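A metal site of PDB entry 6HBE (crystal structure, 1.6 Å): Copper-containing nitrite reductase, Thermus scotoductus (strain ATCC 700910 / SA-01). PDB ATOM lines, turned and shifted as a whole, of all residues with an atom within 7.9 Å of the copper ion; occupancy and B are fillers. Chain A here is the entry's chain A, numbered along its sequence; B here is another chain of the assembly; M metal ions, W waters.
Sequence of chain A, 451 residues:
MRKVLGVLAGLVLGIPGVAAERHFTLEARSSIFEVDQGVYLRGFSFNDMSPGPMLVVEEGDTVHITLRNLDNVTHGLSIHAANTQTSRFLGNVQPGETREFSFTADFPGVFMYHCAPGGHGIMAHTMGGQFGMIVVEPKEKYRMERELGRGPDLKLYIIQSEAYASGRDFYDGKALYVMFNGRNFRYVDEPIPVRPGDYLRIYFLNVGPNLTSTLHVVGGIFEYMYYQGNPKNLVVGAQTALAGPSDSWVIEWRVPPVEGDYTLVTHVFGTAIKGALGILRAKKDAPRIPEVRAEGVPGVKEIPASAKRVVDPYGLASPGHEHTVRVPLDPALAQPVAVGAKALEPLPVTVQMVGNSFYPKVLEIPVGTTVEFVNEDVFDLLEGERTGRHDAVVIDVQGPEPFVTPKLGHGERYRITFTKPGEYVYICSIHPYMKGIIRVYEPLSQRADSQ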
ATOM      1  N   SER A  78     -18.717 -15.553 -29.969  1.00  0.00           N
ATOM      2  CA  SER A  78     -19.067 -14.223 -29.527  1.00  0.00           C
ATOM      3  C   SER A  78     -18.541 -14.004 -28.115  1.00  0.00           C
ATOM      4  O   SER A  78     -18.611 -14.905 -27.283  1.00  0.00           O
ATOM      5  CB  SER A  78     -20.614 -14.069 -29.552  1.00  0.00           C
ATOM      6  OG  SER A  78     -20.995 -12.846 -28.945  1.00  0.00           O
ATOM      7  N   ILE A  79     -18.047 -12.798 -27.837  1.00  0.00           N
ATOM      8  CA  ILE A  79     -17.400 -12.489 -26.575  1.00  0.00           C
ATOM      9  C   ILE A  79     -17.871 -11.110 -26.073  1.00  0.00           C
ATOM     10  O   ILE A  79     -17.531 -10.058 -26.653  1.00  0.00           O
ATOM     11  CB  ILE A  79     -15.829 -12.654 -26.665  1.00  0.00           C
ATOM     12  CG1 ILE A  79     -15.132 -12.218 -25.373  1.00  0.00           C
ATOM     13  CG2 ILE A  79     -15.234 -11.929 -27.843  1.00  0.00           C
ATOM     14  CD1 ILE A  79     -13.866 -13.035 -25.105  1.00  0.00           C
ATOM     15  N   HIS A  80     -18.691 -11.114 -25.014  1.00  0.00           N
ATOM     16  CA  HIS A  80     -19.465  -9.910 -24.671  1.00  0.00           C
ATOM     17  C   HIS A  80     -18.574  -8.792 -24.095  1.00  0.00           C
ATOM     18  O   HIS A  80     -19.019  -7.654 -23.995  1.00  0.00           O
ATOM     19  CB  HIS A  80     -20.603 -10.227 -23.664  1.00  0.00           C
ATOM     20  CG  HIS A  80     -21.710 -11.051 -24.250  1.00  0.00           C
ATOM     21  ND1 HIS A  80     -22.871 -11.326 -23.545  1.00  0.00           N
ATOM     22  CD2 HIS A  80     -21.863 -11.641 -25.460  1.00  0.00           C
ATOM     23  CE1 HIS A  80     -23.666 -12.081 -24.286  1.00  0.00           C
ATOM     24  NE2 HIS A  80     -23.104 -12.255 -25.471  1.00  0.00           N
ATOM     25  N   MET A 112     -20.354 -12.853 -20.538  1.00  0.00           N
ATOM     26  CA  MET A 112     -20.500 -14.184 -21.195  1.00  0.00           C
ATOM     27  C   MET A 112     -19.675 -14.257 -22.491  1.00  0.00           C
ATOM     28  O   MET A 112     -19.553 -13.260 -23.208  1.00  0.00           O
ATOM     29  CB  MET A 112     -21.993 -14.445 -21.490  1.00  0.00           C
ATOM     30  CG  MET A 112     -22.360 -15.839 -22.022  1.00  0.00           C
ATOM     31  SD  MET A 112     -24.179 -15.956 -22.074  1.00  0.00           S
ATOM     32  CE  MET A 112     -24.379 -17.566 -22.876  1.00  0.00           C
ATOM     33  N   TYR A 113     -19.195 -15.460 -22.830  1.00  0.00           N
ATOM     34  CA  TYR A 113     -18.819 -15.814 -24.209  1.00  0.00           C
ATOM     35  C   TYR A 113     -19.535 -17.124 -24.563  1.00  0.00           C
ATOM     36  O   TYR A 113     -19.925 -17.859 -23.672  1.00  0.00           O
ATOM     37  CB  TYR A 113     -17.277 -15.897 -24.396  1.00  0.00           C
ATOM     38  CG  TYR A 113     -16.585 -17.078 -23.769  1.00  0.00           C
ATOM     39  CD1 TYR A 113     -16.625 -18.336 -24.380  1.00  0.00           C
ATOM     40  CD2 TYR A 113     -15.873 -16.962 -22.576  1.00  0.00           C
ATOM     41  CE1 TYR A 113     -16.007 -19.431 -23.820  1.00  0.00           C
ATOM     42  CE2 TYR A 113     -15.218 -18.050 -22.028  1.00  0.00           C
ATOM     43  CZ  TYR A 113     -15.282 -19.294 -22.653  1.00  0.00           C
ATOM     44  OH  TYR A 113     -14.685 -20.412 -22.143  1.00  0.00           O
ATOM     45  N   HIS A 114     -19.779 -17.337 -25.846  1.00  0.00           N
ATOM     46  CA  HIS A 114     -20.488 -18.527 -26.332  1.00  0.00           C
ATOM     47  C   HIS A 114     -20.218 -18.778 -27.797  1.00  0.00           C
ATOM     48  O   HIS A 114     -19.679 -17.917 -28.489  1.00  0.00           O
ATOM     49  CB  HIS A 114     -22.012 -18.369 -26.063  1.00  0.00           C
ATOM     50  CG  HIS A 114     -22.643 -17.156 -26.687  1.00  0.00           C
ATOM     51  ND1 HIS A 114     -23.090 -17.138 -27.984  1.00  0.00           N
ATOM     52  CD2 HIS A 114     -22.933 -15.924 -26.193  1.00  0.00           C
ATOM     53  CE1 HIS A 114     -23.577 -15.963 -28.287  1.00  0.00           C
ATOM     54  NE2 HIS A 114     -23.515 -15.202 -27.216  1.00  0.00           N
ATOM     55  N   CYS A 115     -20.614 -19.946 -28.300  1.00  0.00           N
ATOM     56  CA  CYS A 115     -20.467 -20.241 -29.734  1.00  0.00           C
ATOM     57  C   CYS A 115     -21.392 -19.327 -30.571  1.00  0.00           C
ATOM     58  O   CYS A 115     -22.506 -18.943 -30.134  1.00  0.00           O
ATOM     59  CB  CYS A 115     -20.721 -21.723 -30.010  1.00  0.00           C
ATOM     60  SG  CYS A 115     -20.182 -22.196 -31.681  1.00  0.00           S
ATOM     61  N   ALA A 116     -20.900 -18.920 -31.733  1.00  0.00           N
ATOM     62  CA  ALA A 116     -21.670 -18.116 -32.700  1.00  0.00           C
ATOM     63  C   ALA A 116     -21.283 -18.526 -34.122  1.00  0.00           C
ATOM     64  O   ALA A 116     -20.584 -17.799 -34.806  1.00  0.00           O
ATOM     65  CB  ALA A 116     -21.432 -16.617 -32.460  1.00  0.00           C
ATOM     66  N   ILE A 122     -26.335 -19.889 -33.473  1.00  0.00           N
ATOM     67  CA  ILE A 122     -25.946 -19.188 -32.243  1.00  0.00           C
ATOM     68  C   ILE A 122     -26.738 -19.772 -31.048  1.00  0.00           C
ATOM     69  O   ILE A 122     -26.176 -20.181 -30.026  1.00  0.00           O
ATOM     70  CB  ILE A 122     -26.227 -17.673 -32.329  1.00  0.00           C
ATOM     71  CG1 ILE A 122     -25.475 -17.014 -33.518  1.00  0.00           C
ATOM     72  CG2 ILE A 122     -25.864 -17.008 -31.023  1.00  0.00           C
ATOM     73  CD1 ILE A 122     -25.845 -15.564 -33.740  1.00  0.00           C
ATOM     74  N   THR A 126     -25.308 -22.807 -28.412  1.00  0.00           N
ATOM     75  CA  THR A 126     -25.181 -22.338 -27.037  1.00  0.00           C
ATOM     76  C   THR A 126     -25.936 -23.217 -26.054  1.00  0.00           C
ATOM     77  O   THR A 126     -25.402 -23.584 -24.986  1.00  0.00           O
ATOM     78  CB  THR A 126     -25.574 -20.859 -26.899  1.00  0.00           C
ATOM     79  OG1 THR A 126     -24.683 -20.050 -27.680  1.00  0.00           O
ATOM     80  CG2 THR A 126     -25.534 -20.420 -25.402  1.00  0.00           C
ATOM     81  N   SER A 246     -27.731 -14.251 -19.484  1.00  0.00           N
ATOM     82  CA  SER A 246     -26.559 -13.421 -19.793  1.00  0.00           C
ATOM     83  C   SER A 246     -26.441 -12.199 -18.861  1.00  0.00           C
ATOM     84  O   SER A 246     -25.554 -11.395 -19.084  1.00  0.00           O
ATOM     85  CB  SER A 246     -26.432 -12.959 -21.263  1.00  0.00           C
ATOM     86  OG  SER A 246     -25.127 -12.412 -21.505  1.00  0.00           O
ATOM     87  N   HIS B 216     -29.722  -7.393 -26.222  1.00  0.00           N
ATOM     88  CA  HIS B 216     -28.265  -7.472 -26.423  1.00  0.00           C
ATOM     89  C   HIS B 216     -27.908  -7.031 -27.853  1.00  0.00           C
ATOM     90  O   HIS B 216     -28.706  -7.271 -28.778  1.00  0.00           O
ATOM     91  CB  HIS B 216     -27.782  -8.900 -26.142  1.00  0.00           C
ATOM     92  CG  HIS B 216     -26.350  -9.178 -26.527  1.00  0.00           C
ATOM     93  ND1 HIS B 216     -25.270  -8.704 -25.797  1.00  0.00           N
ATOM     94  CD2 HIS B 216     -25.835  -9.925 -27.531  1.00  0.00           C
ATOM     95  CE1 HIS B 216     -24.150  -9.128 -26.357  1.00  0.00           C
ATOM     96  NE2 HIS B 216     -24.461  -9.869 -27.419  1.00  0.00           N
ATOM     97  N   VAL B 217     -26.728  -6.429 -28.059  1.00  0.00           N
ATOM     98  CA  VAL B 217     -26.159  -6.223 -29.423  1.00  0.00           C
ATOM     99  C   VAL B 217     -24.798  -6.932 -29.546  1.00  0.00           C
ATOM    100  O   VAL B 217     -23.907  -6.644 -28.765  1.00  0.00           O
ATOM    101  CB  VAL B 217     -25.996  -4.712 -29.806  1.00  0.00           C
ATOM    102  CG1 VAL B 217     -25.321  -4.577 -31.187  1.00  0.00           C
ATOM    103  CG2 VAL B 217     -27.332  -4.013 -29.879  1.00  0.00           C
ATOM    104  N   VAL B 218     -24.680  -7.867 -30.499  1.00  0.00           N
ATOM    105  CA  VAL B 218     -23.425  -8.633 -30.717  1.00  0.00           C
ATOM    106  C   VAL B 218     -22.383  -7.667 -31.275  1.00  0.00           C
ATOM    107  O   VAL B 218     -22.591  -7.067 -32.336  1.00  0.00           O
ATOM    108  CB  VAL B 218     -23.636  -9.800 -31.725  1.00  0.00           C
ATOM    109  CG1 VAL B 218     -22.358 -10.650 -31.860  1.00  0.00           C
ATOM    110  CG2 VAL B 218     -24.807 -10.685 -31.286  1.00  0.00           C
ATOM    111  N   GLY B 219     -21.290  -7.502 -30.534  1.00  0.00           N
ATOM    112  CA  GLY B 219     -20.253  -6.521 -30.859  1.00  0.00           C
ATOM    113  C   GLY B 219     -20.458  -5.197 -30.152  1.00  0.00           C
ATOM    114  O   GLY B 219     -19.761  -4.226 -30.455  1.00  0.00           O
ATOM    115  N   GLN B 239     -23.993  -5.508 -20.968  1.00  0.00           N
ATOM    116  CA  GLN B 239     -24.173  -6.470 -22.071  1.00  0.00           C
ATOM    117  C   GLN B 239     -25.628  -6.846 -22.339  1.00  0.00           C
ATOM    118  O   GLN B 239     -25.931  -7.385 -23.411  1.00  0.00           O
ATOM    119  CB  GLN B 239     -23.327  -7.740 -21.834  1.00  0.00           C
ATOM    120  CG  GLN B 239     -23.942  -8.752 -20.874  1.00  0.00           C
ATOM    121  CD  GLN B 239     -22.901  -9.585 -20.160  1.00  0.00           C
ATOM    122  OE1 GLN B 239     -22.368 -10.549 -20.699  1.00  0.00           O
ATOM    123  NE2 GLN B 239     -22.641  -9.235 -18.918  1.00  0.00           N
ATOM    124  N   THR B 240     -26.507  -6.621 -21.365  1.00  0.00           N
ATOM    125  CA  THR B 240     -27.916  -6.945 -21.433  1.00  0.00           C
ATOM    126  C   THR B 240     -28.776  -5.858 -20.752  1.00  0.00           C
ATOM    127  O   THR B 240     -28.323  -5.209 -19.809  1.00  0.00           O
ATOM    128  CB  THR B 240     -28.243  -8.292 -20.749  1.00  0.00           C
ATOM    129  OG1 THR B 240     -27.537  -8.401 -19.519  1.00  0.00           O
ATOM    130  CG2 THR B 240     -27.935  -9.455 -21.627  1.00  0.00           C
ATOM    131  N   VAL B 265     -30.567  -8.819 -30.412  1.00  0.00           N
ATOM    132  CA  VAL B 265     -31.124 -10.117 -30.022  1.00  0.00           C
ATOM    133  C   VAL B 265     -31.499 -10.078 -28.529  1.00  0.00           C
ATOM    134  O   VAL B 265     -30.938  -9.268 -27.728  1.00  0.00           O
ATOM    135  CB  VAL B 265     -30.126 -11.261 -30.361  1.00  0.00           C
ATOM    136  CG1 VAL B 265     -28.892 -11.216 -29.485  1.00  0.00           C
ATOM    137  CG2 VAL B 265     -30.778 -12.659 -30.330  1.00  0.00           C
ATOM    138  N   THR B 266     -32.463 -10.930 -28.177  1.00  0.00           N
ATOM    139  CA  THR B 266     -32.716 -11.260 -26.764  1.00  0.00           C
ATOM    140  C   THR B 266     -31.875 -12.467 -26.385  1.00  0.00           C
ATOM    141  O   THR B 266     -31.885 -13.512 -27.068  1.00  0.00           O
ATOM    142  CB  THR B 266     -34.216 -11.530 -26.403  1.00  0.00           C
ATOM    143  OG1 THR B 266     -34.274 -12.053 -25.069  1.00  0.00           O
ATOM    144  CG2 THR B 266     -34.891 -12.537 -27.351  1.00  0.00           C
ATOM    145  N   HIS B 267     -31.190 -12.384 -25.261  1.00  0.00           N
ATOM    146  CA  HIS B 267     -30.335 -13.502 -24.817  1.00  0.00           C
ATOM    147  C   HIS B 267     -31.130 -14.651 -24.117  1.00  0.00           C
ATOM    148  O   HIS B 267     -30.541 -15.618 -23.679  1.00  0.00           O
ATOM    149  CB  HIS B 267     -29.125 -13.015 -24.003  1.00  0.00           C
ATOM    150  CG  HIS B 267     -27.816 -13.445 -24.602  1.00  0.00           C
ATOM    151  ND1 HIS B 267     -27.290 -14.693 -24.432  1.00  0.00           N
ATOM    152  CD2 HIS B 267     -26.948 -12.783 -25.424  1.00  0.00           C
ATOM    153  CE1 HIS B 267     -26.143 -14.791 -25.092  1.00  0.00           C
ATOM    154  NE2 HIS B 267     -25.929 -13.645 -25.714  1.00  0.00           N
ATOM    155  N   PHE B 269     -32.578 -17.409 -25.178  1.00  0.00           N
ATOM    156  CA  PHE B 269     -32.336 -17.987 -26.527  1.00  0.00           C
ATOM    157  C   PHE B 269     -33.456 -18.894 -27.026  1.00  0.00           C
ATOM    158  O   PHE B 269     -33.610 -19.026 -28.225  1.00  0.00           O
ATOM    159  CB  PHE B 269     -30.959 -18.667 -26.623  1.00  0.00           C
ATOM    160  CG  PHE B 269     -29.798 -17.757 -26.997  1.00  0.00           C
ATOM    161  CD1 PHE B 269     -29.962 -16.396 -27.331  1.00  0.00           C
ATOM    162  CD2 PHE B 269     -28.520 -18.272 -27.017  1.00  0.00           C
ATOM    163  CE1 PHE B 269     -28.871 -15.598 -27.673  1.00  0.00           C
ATOM    164  CE2 PHE B 269     -27.427 -17.481 -27.383  1.00  0.00           C
ATOM    165  CZ  PHE B 269     -27.597 -16.154 -27.708  1.00  0.00           C
HETATM  166 CU    CU M   1     -24.186 -13.346 -26.775  1.00  0.00          CU
HETATM  167  O   HOH W   1     -23.635 -12.469 -28.466  1.00  0.00           O
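Residues that only touch the copper ion: Ser 78 and His 216 of chain B. Along chain A the residues within 4 Å of the copper ion span positions 78 to 114. The nearest printed residue that does not touch the copper ion is Phe 269 of chain B (4.5 Å).
ND1 of His 216 of chain B lies within hydrogen-bond range of O of Gln 239 of chain B, at 2.8 Å. A ring nitrogen (ND1) of His 80 sits close to the side-chain hydroxyl (OG) of Ser 246. The backbone NH of Ser 78 sits at hydrogen-bond distance from the backbone carbonyl oxygen of His 114, 3.0 Å away. The backbone carbonyl oxygen of Met 112 lies within hydrogen-bond range of the backbone NH of His 80 (2.9 Å). N of His 216 of chain B sits at hydrogen-bond distance from O of Val 265 of chain B (2.7 Å). A ring nitrogen (NE2) of His 80 sits close to a ring nitrogen (NE2) of His 216 of chain B (3.4 Å). OG1 of Thr 126 is in hydrogen-bond range of ND1 of His 114 (3.3 Å). OE1 of Gln 239 of chain B sits at hydrogen-bond distance from ND1 of His 80 (3.0 Å).
The copper ion is bound by water W1, NE2 of His 80, NE2 of His 114 and NE2 of His 267 of chain B. The copper ion has four donor atoms within binding distance.
Water W1 lies within hydrogen-bond range of the side-chain hydroxyl of Ser 78 and a ring nitrogen (NE2) of His 216 of chain B.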
